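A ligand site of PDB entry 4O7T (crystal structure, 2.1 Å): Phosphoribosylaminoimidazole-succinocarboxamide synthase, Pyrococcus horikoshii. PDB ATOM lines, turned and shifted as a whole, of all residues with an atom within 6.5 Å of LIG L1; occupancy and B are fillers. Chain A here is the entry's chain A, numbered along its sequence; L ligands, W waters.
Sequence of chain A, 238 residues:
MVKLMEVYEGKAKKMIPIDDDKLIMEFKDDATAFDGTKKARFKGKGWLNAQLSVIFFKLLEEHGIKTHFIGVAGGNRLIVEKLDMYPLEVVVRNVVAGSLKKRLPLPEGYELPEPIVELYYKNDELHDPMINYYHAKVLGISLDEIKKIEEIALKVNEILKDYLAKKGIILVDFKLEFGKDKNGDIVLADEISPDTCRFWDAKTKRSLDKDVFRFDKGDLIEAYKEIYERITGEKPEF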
ATOM      1  N   GLU A  89     -23.733   1.881  -1.467  1.00  0.00           N
ATOM      2  CA  GLU A  89     -22.668   2.150  -0.524  1.00  0.00           C
ATOM      3  C   GLU A  89     -23.283   1.947   0.864  1.00  0.00           C
ATOM      4  O   GLU A  89     -24.317   2.532   1.180  1.00  0.00           O
ATOM      5  CB  GLU A  89     -22.078   3.548  -0.755  1.00  0.00           C
ATOM      6  CG  GLU A  89     -21.498   3.667  -2.152  1.00  0.00           C
ATOM      7  CD  GLU A  89     -20.794   4.979  -2.460  1.00  0.00           C
ATOM      8  OE1 GLU A  89     -20.576   5.258  -3.665  1.00  0.00           O
ATOM      9  OE2 GLU A  89     -20.438   5.740  -1.529  1.00  0.00           O
ATOM     10  N   VAL A  91     -22.841   2.221   4.764  1.00  0.00           N
ATOM     11  CA  VAL A  91     -22.018   2.973   5.679  1.00  0.00           C
ATOM     12  C   VAL A  91     -22.330   2.543   7.109  1.00  0.00           C
ATOM     13  O   VAL A  91     -23.488   2.532   7.548  1.00  0.00           O
ATOM     14  CB  VAL A  91     -22.202   4.509   5.507  1.00  0.00           C
ATOM     15  CG1 VAL A  91     -21.445   5.288   6.579  1.00  0.00           C
ATOM     16  CG2 VAL A  91     -21.784   4.967   4.113  1.00  0.00           C
ATOM     17  N   VAL A  92     -21.271   2.174   7.846  1.00  0.00           N
ATOM     18  CA  VAL A  92     -21.419   1.845   9.258  1.00  0.00           C
ATOM     19  C   VAL A  92     -20.775   2.955  10.101  1.00  0.00           C
ATOM     20  O   VAL A  92     -19.673   3.413   9.790  1.00  0.00           O
ATOM     21  CB  VAL A  92     -20.797   0.478   9.612  1.00  0.00           C
ATOM     22  CG1 VAL A  92     -21.105   0.110  11.061  1.00  0.00           C
ATOM     23  CG2 VAL A  92     -21.301  -0.614   8.666  1.00  0.00           C
ATOM     24  N   ARG A  93     -21.470   3.388  11.149  1.00  0.00           N
ATOM     25  CA  ARG A  93     -21.048   4.552  11.938  1.00  0.00           C
ATOM     26  C   ARG A  93     -21.074   4.271  13.444  1.00  0.00           C
ATOM     27  O   ARG A  93     -22.088   3.794  13.967  1.00  0.00           O
ATOM     28  CB  ARG A  93     -21.924   5.781  11.582  1.00  0.00           C
ATOM     29  CG  ARG A  93     -22.334   5.861  10.093  1.00  0.00           C
ATOM     30  CD  ARG A  93     -23.146   7.117   9.740  1.00  0.00           C
ATOM     31  NE  ARG A  93     -22.266   8.279   9.631  1.00  0.00           N
ATOM     32  CZ  ARG A  93     -22.009   8.978   8.526  1.00  0.00           C
ATOM     33  NH1 ARG A  93     -22.614   8.707   7.355  1.00  0.00           N
ATOM     34  NH2 ARG A  93     -21.138   9.996   8.610  1.00  0.00           N
ATOM     35  N   ALA A  97     -19.833  11.929  12.961  1.00  0.00           N
ATOM     36  CA  ALA A  97     -18.909  12.691  12.109  1.00  0.00           C
ATOM     37  C   ALA A  97     -19.562  12.893  10.746  1.00  0.00           C
ATOM     38  O   ALA A  97     -20.564  12.260  10.443  1.00  0.00           O
ATOM     39  CB  ALA A  97     -17.601  11.939  11.934  1.00  0.00           C
ATOM     40  N   GLY A  98     -18.982  13.769   9.927  1.00  0.00           N
ATOM     41  CA  GLY A  98     -19.423  13.931   8.536  1.00  0.00           C
ATOM     42  C   GLY A  98     -20.900  14.220   8.378  1.00  0.00           C
ATOM     43  O   GLY A  98     -21.476  15.001   9.155  1.00  0.00           O
ATOM     44  N   SER A  99     -21.535  13.559   7.408  1.00  0.00           N
ATOM     45  CA  SER A  99     -22.937  13.833   7.074  1.00  0.00           C
ATOM     46  C   SER A  99     -23.926  13.485   8.188  1.00  0.00           C
ATOM     47  O   SER A  99     -25.050  14.007   8.226  1.00  0.00           O
ATOM     48  CB  SER A  99     -23.355  13.102   5.780  1.00  0.00           C
ATOM     49  OG  SER A  99     -23.433  11.705   6.025  1.00  0.00           O
ATOM     50  N   LEU A 100     -23.520  12.599   9.112  1.00  0.00           N
ATOM     51  CA  LEU A 100     -24.407  12.248  10.236  1.00  0.00           C
ATOM     52  C   LEU A 100     -24.840  13.453  11.119  1.00  0.00           C
ATOM     53  O   LEU A 100     -25.916  13.430  11.726  1.00  0.00           O
ATOM     54  CB  LEU A 100     -23.819  11.112  11.088  1.00  0.00           C
ATOM     55  CG  LEU A 100     -24.768  10.485  12.119  1.00  0.00           C
ATOM     56  CD1 LEU A 100     -26.033   9.910  11.465  1.00  0.00           C
ATOM     57  CD2 LEU A 100     -24.063   9.416  12.943  1.00  0.00           C
ATOM     58  N   GLU A 118     -26.245   2.903   7.333  1.00  0.00           N
ATOM     59  CA  GLU A 118     -26.937   3.718   6.328  1.00  0.00           C
ATOM     60  C   GLU A 118     -26.730   3.102   4.942  1.00  0.00           C
ATOM     61  O   GLU A 118     -25.645   2.592   4.626  1.00  0.00           O
ATOM     62  CB  GLU A 118     -26.399   5.160   6.336  1.00  0.00           C
ATOM     63  CG  GLU A 118     -26.551   5.887   7.676  1.00  0.00           C
ATOM     64  CD  GLU A 118     -25.915   7.278   7.683  1.00  0.00           C
ATOM     65  OE1 GLU A 118     -25.029   7.562   6.837  1.00  0.00           O
ATOM     66  OE2 GLU A 118     -26.300   8.104   8.547  1.00  0.00           O
ATOM     67  N   TYR A 120     -26.818   3.894   0.840  1.00  0.00           N
ATOM     68  CA  TYR A 120     -26.796   4.921  -0.202  1.00  0.00           C
ATOM     69  C   TYR A 120     -26.872   4.261  -1.570  1.00  0.00           C
ATOM     70  O   TYR A 120     -26.194   3.269  -1.826  1.00  0.00           O
ATOM     71  CB  TYR A 120     -25.538   5.765  -0.106  1.00  0.00           C
ATOM     72  CG  TYR A 120     -25.497   6.624   1.121  1.00  0.00           C
ATOM     73  CD1 TYR A 120     -26.015   7.911   1.116  1.00  0.00           C
ATOM     74  CD2 TYR A 120     -24.953   6.130   2.316  1.00  0.00           C
ATOM     75  CE1 TYR A 120     -25.978   8.712   2.249  1.00  0.00           C
ATOM     76  CE2 TYR A 120     -24.919   6.905   3.469  1.00  0.00           C
ATOM     77  CZ  TYR A 120     -25.426   8.199   3.431  1.00  0.00           C
ATOM     78  OH  TYR A 120     -25.383   8.970   4.580  1.00  0.00           O
ATOM     79  N   ASP A 128     -25.699   9.854  -5.362  1.00  0.00           N
ATOM     80  CA  ASP A 128     -25.656   8.876  -4.263  1.00  0.00           C
ATOM     81  C   ASP A 128     -26.600   9.174  -3.090  1.00  0.00           C
ATOM     82  O   ASP A 128     -26.141   9.362  -1.954  1.00  0.00           O
ATOM     83  CB  ASP A 128     -24.214   8.689  -3.793  1.00  0.00           C
ATOM     84  CG  ASP A 128     -23.290   8.209  -4.903  1.00  0.00           C
ATOM     85  OD1 ASP A 128     -23.762   7.672  -5.917  1.00  0.00           O
ATOM     86  OD2 ASP A 128     -22.069   8.383  -4.781  1.00  0.00           O
ATOM     87  N   ASP A 173     -16.297   5.715  11.386  1.00  0.00           N
ATOM     88  CA  ASP A 173     -17.303   5.264  10.422  1.00  0.00           C
ATOM     89  C   ASP A 173     -16.583   4.742   9.198  1.00  0.00           C
ATOM     90  O   ASP A 173     -15.365   4.909   9.107  1.00  0.00           O
ATOM     91  CB  ASP A 173     -18.346   6.368  10.078  1.00  0.00           C
ATOM     92  CG  ASP A 173     -17.718   7.645   9.490  1.00  0.00           C
ATOM     93  OD1 ASP A 173     -16.758   7.573   8.725  1.00  0.00           O
ATOM     94  OD2 ASP A 173     -18.216   8.743   9.778  1.00  0.00           O
ATOM     95  N   PHE A 174     -17.288   4.095   8.269  1.00  0.00           N
ATOM     96  CA  PHE A 174     -16.651   3.577   7.047  1.00  0.00           C
ATOM     97  C   PHE A 174     -17.675   3.129   6.022  1.00  0.00           C
ATOM     98  O   PHE A 174     -18.828   2.863   6.358  1.00  0.00           O
ATOM     99  CB  PHE A 174     -15.676   2.415   7.363  1.00  0.00           C
ATOM    100  CG  PHE A 174     -16.334   1.193   7.958  1.00  0.00           C
ATOM    101  CD1 PHE A 174     -16.707   0.120   7.154  1.00  0.00           C
ATOM    102  CD2 PHE A 174     -16.565   1.108   9.332  1.00  0.00           C
ATOM    103  CE1 PHE A 174     -17.312  -1.015   7.696  1.00  0.00           C
ATOM    104  CE2 PHE A 174     -17.162  -0.016   9.880  1.00  0.00           C
ATOM    105  CZ  PHE A 174     -17.545  -1.078   9.068  1.00  0.00           C
ATOM    106  N   LYS A 175     -17.238   3.027   4.775  1.00  0.00           N
ATOM    107  CA  LYS A 175     -18.123   2.657   3.683  1.00  0.00           C
ATOM    108  C   LYS A 175     -17.703   1.310   3.078  1.00  0.00           C
ATOM    109  O   LYS A 175     -16.507   1.085   2.774  1.00  0.00           O
ATOM    110  CB  LYS A 175     -18.114   3.749   2.599  1.00  0.00           C
ATOM    111  CG  LYS A 175     -19.102   3.507   1.446  1.00  0.00           C
ATOM    112  CD  LYS A 175     -18.502   2.717   0.271  1.00  0.00           C
ATOM    113  CE  LYS A 175     -17.484   3.547  -0.536  1.00  0.00           C
ATOM    114  NZ  LYS A 175     -16.697   2.711  -1.493  1.00  0.00           N
ATOM    115  N   LEU A 176     -18.690   0.425   2.881  1.00  0.00           N
ATOM    116  CA  LEU A 176     -18.481  -0.846   2.200  1.00  0.00           C
ATOM    117  C   LEU A 176     -19.316  -0.979   0.928  1.00  0.00           C
ATOM    118  O   LEU A 176     -20.356  -0.329   0.765  1.00  0.00           O
ATOM    119  CB  LEU A 176     -18.845  -2.019   3.104  1.00  0.00           C
ATOM    120  CG  LEU A 176     -18.179  -2.146   4.467  1.00  0.00           C
ATOM    121  CD1 LEU A 176     -18.764  -3.358   5.194  1.00  0.00           C
ATOM    122  CD2 LEU A 176     -16.655  -2.240   4.338  1.00  0.00           C
ATOM    123  N   ASP A 195      -9.212   6.149   2.501  1.00  0.00           N
ATOM    124  CA  ASP A 195     -10.168   6.839   1.605  1.00  0.00           C
ATOM    125  C   ASP A 195     -11.629   6.571   1.990  1.00  0.00           C
ATOM    126  O   ASP A 195     -12.490   7.436   1.824  1.00  0.00           O
ATOM    127  CB  ASP A 195      -9.994   6.428   0.122  1.00  0.00           C
ATOM    128  CG  ASP A 195      -8.869   7.192  -0.581  1.00  0.00           C
ATOM    129  OD1 ASP A 195      -8.813   7.189  -1.827  1.00  0.00           O
ATOM    130  OD2 ASP A 195      -8.014   7.784   0.098  1.00  0.00           O
ATOM    131  N   THR A 196     -11.896   5.366   2.493  1.00  0.00           N
ATOM    132  CA  THR A 196     -13.278   4.910   2.689  1.00  0.00           C
ATOM    133  C   THR A 196     -13.663   4.662   4.160  1.00  0.00           C
ATOM    134  O   THR A 196     -14.748   4.135   4.450  1.00  0.00           O
ATOM    135  CB  THR A 196     -13.572   3.657   1.828  1.00  0.00           C
ATOM    136  OG1 THR A 196     -12.655   2.614   2.177  1.00  0.00           O
ATOM    137  CG2 THR A 196     -13.402   3.983   0.342  1.00  0.00           C
ATOM    138  N   CYS A 197     -12.773   5.081   5.071  1.00  0.00           N
ATOM    139  CA  CYS A 197     -13.013   4.996   6.524  1.00  0.00           C
ATOM    140  C   CYS A 197     -12.615   6.302   7.201  1.00  0.00           C
ATOM    141  O   CYS A 197     -11.802   7.064   6.658  1.00  0.00           O
ATOM    142  CB  CYS A 197     -12.166   3.887   7.184  1.00  0.00           C
ATOM    143  SG  CYS A 197     -12.197   2.241   6.423  1.00  0.00           S
ATOM    144  N   ARG A 198     -13.170   6.542   8.372  1.00  0.00           N
ATOM    145  CA  ARG A 198     -12.636   7.548   9.293  1.00  0.00           C
ATOM    146  C   ARG A 198     -11.853   6.851  10.407  1.00  0.00           C
ATOM    147  O   ARG A 198     -12.369   5.955  11.082  1.00  0.00           O
ATOM    148  CB  ARG A 198     -13.723   8.492   9.828  1.00  0.00           C
ATOM    149  CG  ARG A 198     -14.211   9.510   8.783  1.00  0.00           C
ATOM    150  CD  ARG A 198     -15.090  10.609   9.381  1.00  0.00           C
ATOM    151  NE  ARG A 198     -15.445  11.606   8.354  1.00  0.00           N
ATOM    152  CZ  ARG A 198     -16.602  11.638   7.703  1.00  0.00           C
ATOM    153  NH1 ARG A 198     -17.573  10.768   7.974  1.00  0.00           N
ATOM    154  NH2 ARG A 198     -16.816  12.573   6.793  1.00  0.00           N
ATOM    155  N   LYS A 210      -8.874  10.354   4.910  1.00  0.00           N
ATOM    156  CA  LYS A 210      -9.114  11.279   3.815  1.00  0.00           C
ATOM    157  C   LYS A 210      -9.621  12.666   4.261  1.00  0.00           C
ATOM    158  O   LYS A 210      -9.524  13.626   3.498  1.00  0.00           O
ATOM    159  CB  LYS A 210     -10.075  10.651   2.801  1.00  0.00           C
ATOM    160  CG  LYS A 210     -10.268  11.405   1.509  1.00  0.00           C
ATOM    161  CD  LYS A 210     -10.958  10.523   0.478  1.00  0.00           C
ATOM    162  CE  LYS A 210     -11.585  11.369  -0.598  1.00  0.00           C
ATOM    163  NZ  LYS A 210     -12.389  10.573  -1.552  1.00  0.00           N
ATOM    164  N   ASP A 211     -10.116  12.759   5.498  1.00  0.00           N
ATOM    165  CA  ASP A 211     -10.575  14.037   6.070  1.00  0.00           C
ATOM    166  C   ASP A 211      -9.452  15.070   6.149  1.00  0.00           C
ATOM    167  O   ASP A 211      -9.706  16.273   6.070  1.00  0.00           O
ATOM    168  CB  ASP A 211     -11.208  13.850   7.455  1.00  0.00           C
ATOM    169  CG  ASP A 211     -12.702  13.473   7.405  1.00  0.00           C
ATOM    170  OD1 ASP A 211     -13.355  13.546   6.334  1.00  0.00           O
ATOM    171  OD2 ASP A 211     -13.241  13.118   8.467  1.00  0.00           O
ATOM    172  N   ARG A 214      -9.830  16.313   2.767  1.00  0.00           N
ATOM    173  CA  ARG A 214     -11.136  16.965   2.638  1.00  0.00           C
ATOM    174  C   ARG A 214     -11.158  18.364   3.270  1.00  0.00           C
ATOM    175  O   ARG A 214     -11.710  19.287   2.694  1.00  0.00           O
ATOM    176  CB  ARG A 214     -12.255  16.095   3.217  1.00  0.00           C
ATOM    177  CG  ARG A 214     -12.617  14.865   2.392  1.00  0.00           C
ATOM    178  CD  ARG A 214     -13.849  14.186   2.976  1.00  0.00           C
ATOM    179  NE  ARG A 214     -14.080  12.845   2.441  1.00  0.00           N
ATOM    180  CZ  ARG A 214     -13.791  11.708   3.073  1.00  0.00           C
ATOM    181  NH1 ARG A 214     -14.055  10.555   2.482  1.00  0.00           N
ATOM    182  NH2 ARG A 214     -13.253  11.717   4.294  1.00  0.00           N
HETATM  183  P1  LIG L   1     -20.189  10.745   5.152  1.00  0.00           P
HETATM  184  O1  LIG L   1     -19.749  11.621   4.038  1.00  0.00           O
HETATM  185  O2  LIG L   1     -21.561  10.151   4.929  1.00  0.00           O
HETATM  186  O3  LIG L   1     -19.943  11.267   6.552  1.00  0.00           O
HETATM  187  O4  LIG L   1     -19.154   9.521   5.024  1.00  0.00           O
HETATM  188  C1  LIG L   1     -19.246   8.352   5.853  1.00  0.00           C
HETATM  189  C2  LIG L   1     -18.074   7.424   5.562  1.00  0.00           C
HETATM  190  O5  LIG L   1     -18.200   6.848   4.255  1.00  0.00           O
HETATM  191  C3  LIG L   1     -16.709   8.124   5.598  1.00  0.00           C
HETATM  192  O6  LIG L   1     -15.817   7.262   6.296  1.00  0.00           O
HETATM  193  C4  LIG L   1     -16.178   8.153   4.192  1.00  0.00           C
HETATM  194  C5  LIG L   1     -17.036   7.125   3.453  1.00  0.00           C
HETATM  195  N1  LIG L   1     -17.404   7.600   2.116  1.00  0.00           N
HETATM  196  C6  LIG L   1     -16.858   6.979   0.962  1.00  0.00           C
HETATM  197  O7  LIG L   1     -16.046   6.040   1.103  1.00  0.00           O
HETATM  198  N2  LIG L   1     -17.186   7.382  -0.276  1.00  0.00           N
HETATM  199  C7  LIG L   1     -18.038   8.405  -0.458  1.00  0.00           C
HETATM  200  O8  LIG L   1     -18.327   8.797  -1.610  1.00  0.00           O
HETATM  201  C8  LIG L   1     -18.642   9.086   0.719  1.00  0.00           C
HETATM  202  C9  LIG L   1     -19.624  10.237   0.566  1.00  0.00           C
HETATM  203  C10 LIG L   1     -18.286   8.632   1.987  1.00  0.00           C
HETATM  204  N1  LG2 L   2     -16.034  14.055   0.113  1.00  0.00           N
HETATM  205  C1  LG2 L   2     -16.675  12.842  -0.481  1.00  0.00           C
HETATM  206  C2  LG2 L   2     -15.696  11.699  -0.700  1.00  0.00           C
HETATM  207  O1  LG2 L   2     -15.114  11.566  -1.779  1.00  0.00           O
HETATM  208  C3  LG2 L   2     -17.381  13.166  -1.801  1.00  0.00           C
HETATM  209  C4  LG2 L   2     -18.767  13.730  -1.597  1.00  0.00           C
HETATM  210  O2  LG2 L   2     -19.625  13.531  -2.493  1.00  0.00           O
HETATM  211  O3  LG2 L   2     -19.016  14.384  -0.564  1.00  0.00           O
HETATM  212  O4  LG2 L   2     -15.489  10.869   0.192  1.00  0.00           O
HETATM  213  O   HOH W   1     -21.600  12.624   2.301  1.00  0.00           O
HETATM  214  O   HOH W   2     -21.212   8.660  -2.295  1.00  0.00           O
HETATM  215  O   HOH W   3     -17.570  11.821   2.558  1.00  0.00           O
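Water W3 lies within hydrogen-bond range of O1 of LIG L1 (2.6 Å) and O4 of LG2 L2 (3.3 Å).
The side-chain carboxylate (OD2) of Asp 211 lies within salt-bridge range of the guanidinium group (NE) of Arg 198. The side-chain carboxylate (OD2) of Asp 173 is in salt-bridge range of the guanidinium group (NH2) of Arg 93. OG of Ser 99 lies within hydrogen-bond range of NH1 of Arg 93. O of Thr 196 is in hydrogen-bond range of N of Lys 175, 2.7 Å away. The backbone NH of Phe 174 lies within hydrogen-bond range of the backbone carbonyl oxygen of Val 92 (2.9 Å). The guanidinium group of Arg 93 is in hydrogen-bond range of the backbone carbonyl oxygen of Ala 97 (3.0 Å). The backbone carbonyl oxygen of Val 91 is in hydrogen-bond range of the backbone NH of Glu 118, at 2.8 Å. The guanidinium group (NH2) of Arg 214 is in salt-bridge range of the side-chain carboxylate (OD1) of Asp 211 (2.7 Å).
Glu 89 touches LIG L1 (OE2 to O8, 3.7 Å). Val 91 touches LIG L1 (CG1 to C1, 3.8 Å). Gly 98 touches LIG L1 (CA to O3, 3.4 Å). Phe 174 touches LIG L1. Lys 175 touches LIG L1 (CE to O7, 3.3 Å). Asp 195 touches LIG L1 (O to O7, 3.9 Å). Thr 196 touches LIG L1. Cys 197 touches LIG L1 (C to O6, 3.5 Å). NH1 of Arg 214 touches C4 of LIG L1 (3.6 Å). Of the 22 residues printed, 13 come within 4 Å of LIG L1.
The side-chain hydroxyl (OG) of Ser 99 lies within hydrogen-bond range of an oxygen (O2) of LIG L1, at 2.7 Å. The guanidinium group (NH2) of Arg 93 is in salt-bridge range of an oxygen (O3) of LIG L1. O3 of LIG L1 is in salt-bridge range of NH1 of Arg 198, at 2.8 Å. An oxygen (O1) of LG2 L2 lies within salt-bridge range of the side-chain amino group (NZ) of Lys 210 (2.9 Å). The backbone NH of Arg 198 is in hydrogen-bond range of an oxygen (O6) of LIG L1 (3.4 Å). An oxygen (O3) of LIG L1 lies within hydrogen-bond range of the backbone NH (N) of Ser 99. An oxygen (O4) of LG2 L2 is in salt-bridge range of the guanidinium group (NH1) of Arg 214 (2.7 Å). OD1 of Asp 173 lies within hydrogen-bond range of O6 of LIG L1 (2.6 Å).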
